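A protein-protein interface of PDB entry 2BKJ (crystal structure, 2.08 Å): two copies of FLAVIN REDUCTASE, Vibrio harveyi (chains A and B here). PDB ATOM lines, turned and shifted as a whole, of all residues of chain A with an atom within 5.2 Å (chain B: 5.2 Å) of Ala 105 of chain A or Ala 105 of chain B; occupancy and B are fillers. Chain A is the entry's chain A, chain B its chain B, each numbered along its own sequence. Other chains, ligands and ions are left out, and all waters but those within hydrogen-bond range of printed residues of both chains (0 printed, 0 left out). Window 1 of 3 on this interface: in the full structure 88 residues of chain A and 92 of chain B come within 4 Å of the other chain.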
ATOM      1  N   ILE A  81     -15.287 -32.805   7.617  1.00  0.00           N
ATOM      2  CA  ILE A  81     -14.354 -31.795   8.099  1.00  0.00           C
ATOM      3  C   ILE A  81     -13.011 -32.344   7.618  1.00  0.00           C
ATOM      4  O   ILE A  81     -12.761 -33.547   7.728  1.00  0.00           O
ATOM      5  CB  ILE A  81     -14.331 -31.728   9.638  1.00  0.00           C
ATOM      6  CG1 ILE A  81     -15.706 -31.323  10.172  1.00  0.00           C
ATOM      7  CG2 ILE A  81     -13.269 -30.744  10.100  1.00  0.00           C
ATOM      8  CD1 ILE A  81     -15.796 -31.295  11.688  1.00  0.00           C
ATOM      9  N   LEU A 100     -11.654 -25.220  15.557  1.00  0.00           N
ATOM     10  CA  LEU A 100     -11.528 -25.756  14.206  1.00  0.00           C
ATOM     11  C   LEU A 100     -12.661 -26.711  13.829  1.00  0.00           C
ATOM     12  O   LEU A 100     -13.027 -26.821  12.658  1.00  0.00           O
ATOM     13  CB  LEU A 100     -10.155 -26.412  14.037  1.00  0.00           C
ATOM     14  CG  LEU A 100      -9.002 -25.454  14.364  1.00  0.00           C
ATOM     15  CD1 LEU A 100      -7.668 -26.150  14.199  1.00  0.00           C
ATOM     16  CD2 LEU A 100      -9.079 -24.218  13.474  1.00  0.00           C
ATOM     17  N   THR A 101     -13.215 -27.399  14.823  1.00  0.00           N
ATOM     18  CA  THR A 101     -14.335 -28.303  14.589  1.00  0.00           C
ATOM     19  C   THR A 101     -15.580 -27.451  14.325  1.00  0.00           C
ATOM     20  O   THR A 101     -16.411 -27.802  13.483  1.00  0.00           O
ATOM     21  CB  THR A 101     -14.561 -29.250  15.788  1.00  0.00           C
ATOM     22  OG1 THR A 101     -13.480 -30.189  15.853  1.00  0.00           O
ATOM     23  CG2 THR A 101     -15.875 -30.012  15.649  1.00  0.00           C
ATOM     24  N   LEU A 102     -15.686 -26.321  15.028  1.00  0.00           N
ATOM     25  CA  LEU A 102     -16.806 -25.398  14.846  1.00  0.00           C
ATOM     26  C   LEU A 102     -16.755 -24.833  13.433  1.00  0.00           C
ATOM     27  O   LEU A 102     -17.781 -24.725  12.761  1.00  0.00           O
ATOM     28  CB  LEU A 102     -16.745 -24.242  15.847  1.00  0.00           C
ATOM     29  CG  LEU A 102     -17.099 -24.485  17.315  1.00  0.00           C
ATOM     30  CD1 LEU A 102     -17.157 -23.138  18.028  1.00  0.00           C
ATOM     31  CD2 LEU A 102     -18.442 -25.195  17.435  1.00  0.00           C
ATOM     32  N   ILE A 103     -15.552 -24.465  12.994  1.00  0.00           N
ATOM     33  CA  ILE A 103     -15.349 -23.925  11.654  1.00  0.00           C
ATOM     34  C   ILE A 103     -15.735 -24.974  10.613  1.00  0.00           C
ATOM     35  O   ILE A 103     -16.442 -24.672   9.648  1.00  0.00           O
ATOM     36  CB  ILE A 103     -13.880 -23.482  11.439  1.00  0.00           C
ATOM     37  CG1 ILE A 103     -13.586 -22.230  12.272  1.00  0.00           C
ATOM     38  CG2 ILE A 103     -13.602 -23.221   9.957  1.00  0.00           C
ATOM     39  CD1 ILE A 103     -12.168 -21.705  12.122  1.00  0.00           C
ATOM     40  N   GLY A 104     -15.291 -26.210  10.834  1.00  0.00           N
ATOM     41  CA  GLY A 104     -15.611 -27.289   9.916  1.00  0.00           C
ATOM     42  C   GLY A 104     -17.108 -27.495   9.800  1.00  0.00           C
ATOM     43  O   GLY A 104     -17.627 -27.678   8.702  1.00  0.00           O
ATOM     44  N   ALA A 105     -17.806 -27.430  10.932  1.00  0.00           N
ATOM     45  CA  ALA A 105     -19.254 -27.610  10.972  1.00  0.00           C
ATOM     46  C   ALA A 105     -20.014 -26.458  10.313  1.00  0.00           C
ATOM     47  O   ALA A 105     -20.922 -26.686   9.510  1.00  0.00           O
ATOM     48  CB  ALA A 105     -19.719 -27.795  12.410  1.00  0.00           C
ATOM     49  N   VAL A 106     -19.657 -25.224  10.666  1.00  0.00           N
ATOM     50  CA  VAL A 106     -20.309 -24.047  10.094  1.00  0.00           C
ATOM     51  C   VAL A 106     -20.069 -23.962   8.588  1.00  0.00           C
ATOM     52  O   VAL A 106     -21.017 -23.846   7.813  1.00  0.00           O
ATOM     53  CB  VAL A 106     -19.822 -22.741  10.775  1.00  0.00           C
ATOM     54  CG1 VAL A 106     -20.381 -21.514  10.049  1.00  0.00           C
ATOM     55  CG2 VAL A 106     -20.263 -22.718  12.236  1.00  0.00           C
ATOM     56  N   ASP A 107     -18.805 -24.041   8.179  1.00  0.00           N
ATOM     57  CA  ASP A 107     -18.445 -23.971   6.763  1.00  0.00           C
ATOM     58  C   ASP A 107     -19.056 -25.088   5.913  1.00  0.00           C
ATOM     59  O   ASP A 107     -19.328 -24.883   4.728  1.00  0.00           O
ATOM     60  CB  ASP A 107     -16.923 -23.934   6.594  1.00  0.00           C
ATOM     61  CG  ASP A 107     -16.318 -22.585   6.982  1.00  0.00           C
ATOM     62  OD1 ASP A 107     -16.991 -21.780   7.665  1.00  0.00           O
ATOM     63  OD2 ASP A 107     -15.158 -22.329   6.596  1.00  0.00           O
ATOM     64  N   SER A 108     -19.259 -26.264   6.510  1.00  0.00           N
ATOM     65  CA  SER A 108     -19.872 -27.394   5.808  1.00  0.00           C
ATOM     66  C   SER A 108     -21.335 -27.078   5.521  1.00  0.00           C
ATOM     67  O   SER A 108     -21.822 -27.319   4.417  1.00  0.00           O
ATOM     68  CB  SER A 108     -19.793 -28.677   6.646  1.00  0.00           C
ATOM     69  OG  SER A 108     -18.480 -29.212   6.662  1.00  0.00           O
ATOM     70  N   GLY A 109     -22.031 -26.551   6.531  1.00  0.00           N
ATOM     71  CA  GLY A 109     -23.433 -26.198   6.374  1.00  0.00           C
ATOM     72  C   GLY A 109     -23.616 -25.160   5.283  1.00  0.00           C
ATOM     73  O   GLY A 109     -24.519 -25.266   4.457  1.00  0.00           O
ATOM     74  N   LEU A 152     -19.777 -35.521   8.943  1.00  0.00           N
ATOM     75  CA  LEU A 152     -20.790 -34.674   9.557  1.00  0.00           C
ATOM     76  C   LEU A 152     -22.191 -35.034   9.085  1.00  0.00           C
ATOM     77  O   LEU A 152     -23.096 -35.211   9.897  1.00  0.00           O
ATOM     78  CB  LEU A 152     -20.517 -33.197   9.270  1.00  0.00           C
ATOM     79  CG  LEU A 152     -19.328 -32.534   9.966  1.00  0.00           C
ATOM     80  CD1 LEU A 152     -19.287 -31.069   9.561  1.00  0.00           C
ATOM     81  CD2 LEU A 152     -19.451 -32.661  11.487  1.00  0.00           C
ATOM     82  N   ILE B  81     -26.421 -20.459  18.795  1.00  0.00           N
ATOM     83  CA  ILE B  81     -26.947 -21.798  19.042  1.00  0.00           C
ATOM     84  C   ILE B  81     -27.955 -21.544  20.162  1.00  0.00           C
ATOM     85  O   ILE B  81     -27.641 -20.838  21.122  1.00  0.00           O
ATOM     86  CB  ILE B  81     -25.857 -22.755  19.573  1.00  0.00           C
ATOM     87  CG1 ILE B  81     -24.793 -22.992  18.502  1.00  0.00           C
ATOM     88  CG2 ILE B  81     -26.482 -24.076  20.016  1.00  0.00           C
ATOM     89  CD1 ILE B  81     -23.682 -23.932  18.936  1.00  0.00           C
ATOM     90  N   THR B 101     -24.149 -29.443  19.804  1.00  0.00           N
ATOM     91  CA  THR B 101     -23.364 -28.275  19.403  1.00  0.00           C
ATOM     92  C   THR B 101     -23.035 -28.376  17.911  1.00  0.00           C
ATOM     93  O   THR B 101     -22.984 -27.363  17.211  1.00  0.00           O
ATOM     94  CB  THR B 101     -22.061 -28.139  20.234  1.00  0.00           C
ATOM     95  OG1 THR B 101     -22.394 -27.746  21.570  1.00  0.00           O
ATOM     96  CG2 THR B 101     -21.129 -27.090  19.633  1.00  0.00           C
ATOM     97  N   LEU B 102     -22.828 -29.601  17.429  1.00  0.00           N
ATOM     98  CA  LEU B 102     -22.542 -29.829  16.017  1.00  0.00           C
ATOM     99  C   LEU B 102     -23.784 -29.476  15.205  1.00  0.00           C
ATOM    100  O   LEU B 102     -23.684 -28.872  14.141  1.00  0.00           O
ATOM    101  CB  LEU B 102     -22.165 -31.287  15.756  1.00  0.00           C
ATOM    102  CG  LEU B 102     -20.828 -31.807  16.279  1.00  0.00           C
ATOM    103  CD1 LEU B 102     -20.631 -33.237  15.788  1.00  0.00           C
ATOM    104  CD2 LEU B 102     -19.694 -30.919  15.786  1.00  0.00           C
ATOM    105  N   ILE B 103     -24.948 -29.870  15.716  1.00  0.00           N
ATOM    106  CA  ILE B 103     -26.226 -29.588  15.063  1.00  0.00           C
ATOM    107  C   ILE B 103     -26.444 -28.078  14.993  1.00  0.00           C
ATOM    108  O   ILE B 103     -26.875 -27.549  13.969  1.00  0.00           O
ATOM    109  CB  ILE B 103     -27.403 -30.250  15.831  1.00  0.00           C
ATOM    110  CG1 ILE B 103     -27.378 -31.767  15.630  1.00  0.00           C
ATOM    111  CG2 ILE B 103     -28.742 -29.668  15.383  1.00  0.00           C
ATOM    112  CD1 ILE B 103     -28.484 -32.509  16.357  1.00  0.00           C
ATOM    113  N   GLY B 104     -26.121 -27.392  16.085  1.00  0.00           N
ATOM    114  CA  GLY B 104     -26.279 -25.950  16.137  1.00  0.00           C
ATOM    115  C   GLY B 104     -25.388 -25.233  15.142  1.00  0.00           C
ATOM    116  O   GLY B 104     -25.835 -24.317  14.456  1.00  0.00           O
ATOM    117  N   ALA B 105     -24.132 -25.665  15.054  1.00  0.00           N
ATOM    118  CA  ALA B 105     -23.164 -25.069  14.140  1.00  0.00           C
ATOM    119  C   ALA B 105     -23.544 -25.302  12.678  1.00  0.00           C
ATOM    120  O   ALA B 105     -23.551 -24.368  11.875  1.00  0.00           O
ATOM    121  CB  ALA B 105     -21.775 -25.618  14.422  1.00  0.00           C
ATOM    122  N   VAL B 106     -23.871 -26.548  12.344  1.00  0.00           N
ATOM    123  CA  VAL B 106     -24.259 -26.904  10.983  1.00  0.00           C
ATOM    124  C   VAL B 106     -25.523 -26.167  10.550  1.00  0.00           C
ATOM    125  O   VAL B 106     -25.537 -25.522   9.503  1.00  0.00           O
ATOM    126  CB  VAL B 106     -24.483 -28.430  10.838  1.00  0.00           C
ATOM    127  CG1 VAL B 106     -25.075 -28.758   9.469  1.00  0.00           C
ATOM    128  CG2 VAL B 106     -23.170 -29.171  11.030  1.00  0.00           C
ATOM    129  N   ASP B 107     -26.573 -26.254  11.365  1.00  0.00           N
ATOM    130  CA  ASP B 107     -27.844 -25.599  11.058  1.00  0.00           C
ATOM    131  C   ASP B 107     -27.721 -24.082  10.944  1.00  0.00           C
ATOM    132  O   ASP B 107     -28.429 -23.462  10.152  1.00  0.00           O
ATOM    133  CB  ASP B 107     -28.919 -25.987  12.080  1.00  0.00           C
ATOM    134  CG  ASP B 107     -29.417 -27.422  11.899  1.00  0.00           C
ATOM    135  OD1 ASP B 107     -28.720 -28.238  11.256  1.00  0.00           O
ATOM    136  OD2 ASP B 107     -30.513 -27.738  12.401  1.00  0.00           O
ATOM    137  N   SER B 108     -26.815 -23.493  11.722  1.00  0.00           N
ATOM    138  CA  SER B 108     -26.586 -22.050  11.681  1.00  0.00           C
ATOM    139  C   SER B 108     -26.002 -21.659  10.331  1.00  0.00           C
ATOM    140  O   SER B 108     -26.429 -20.678   9.725  1.00  0.00           O
ATOM    141  CB  SER B 108     -25.628 -21.619  12.794  1.00  0.00           C
ATOM    142  OG  SER B 108     -26.240 -21.730  14.066  1.00  0.00           O
ATOM    143  N   GLY B 109     -25.019 -22.433   9.871  1.00  0.00           N
ATOM    144  CA  GLY B 109     -24.388 -22.169   8.590  1.00  0.00           C
ATOM    145  C   GLY B 109     -25.379 -22.251   7.443  1.00  0.00           C
ATOM    146  O   GLY B 109     -25.357 -21.420   6.536  1.00  0.00           O
ATOM    147  N   LEU B 152     -21.952 -17.809  17.659  1.00  0.00           N
ATOM    148  CA  LEU B 152     -21.108 -18.487  16.679  1.00  0.00           C
ATOM    149  C   LEU B 152     -20.422 -17.510  15.726  1.00  0.00           C
ATOM    150  O   LEU B 152     -19.202 -17.556  15.554  1.00  0.00           O
ATOM    151  CB  LEU B 152     -21.924 -19.500  15.873  1.00  0.00           C
ATOM    152  CG  LEU B 152     -22.424 -20.748  16.603  1.00  0.00           C
ATOM    153  CD1 LEU B 152     -23.228 -21.606  15.644  1.00  0.00           C
ATOM    154  CD2 LEU B 152     -21.243 -21.530  17.158  1.00  0.00           C
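Among the printed residues, merely in contact across the chains: Ala 105 of chain A with Ala 105 of chain B, Ala 105 of chain A with Val 106 of chain B, Val 106 of chain A with Ala 105 of chain B, Gly 109 of chain A with Val 106 of chain B, Val 106 of chain A with Gly 109 of chain B, Thr 101 of chain A with Leu 102 of chain B and Leu 102 of chain A with Thr 101 of chain B.
Ala 105 of chain A touches two residues of chain B.
Of the printed residues of chain B, Gly 109 of chain A touches Val 106 (3.8 Å).
Printed residues of chain A within 4 Å of Leu 102 of chain B: Thr 101 (3.9 Å).
Ala 105 of chain B touches just these residues of chain A: Ala 105 (3.6 Å) and Val 106 (3.7 Å).
Of the printed residues of chain A, Gly 109 of chain B touches Val 106.
The nearest residue of chain B that does not touch Ala 105 of chain A is Leu 102 of chain B (4.5 Å).
Hydrophobic or aromatic side chains of chain B within 4 Å of the printed part of chain A: Leu 102, Ala 105 and Val 106.
Among the printed residues, 7 pairs touch across the chains.
Thr 101 of chain A touches Leu 102 of chain B, and with the chains exchanged Leu 102 of chain A touches Thr 101 of chain B.
Ala 105 of chain B touches its own counterpart, Ala 105 of chain A.
Ala 105 of chain A touches Val 106 of chain B, and with the chains exchanged Val 106 of chain A touches Ala 105 of chain B.
Val 106 of chain A touches Gly 109 of chain B, and with the chains exchanged Gly 109 of chain A touches Val 106 of chain B.
Of the 7 pairs that touch across the chains among the printed residues, 7 have their exchanged pair printed and touching as well.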
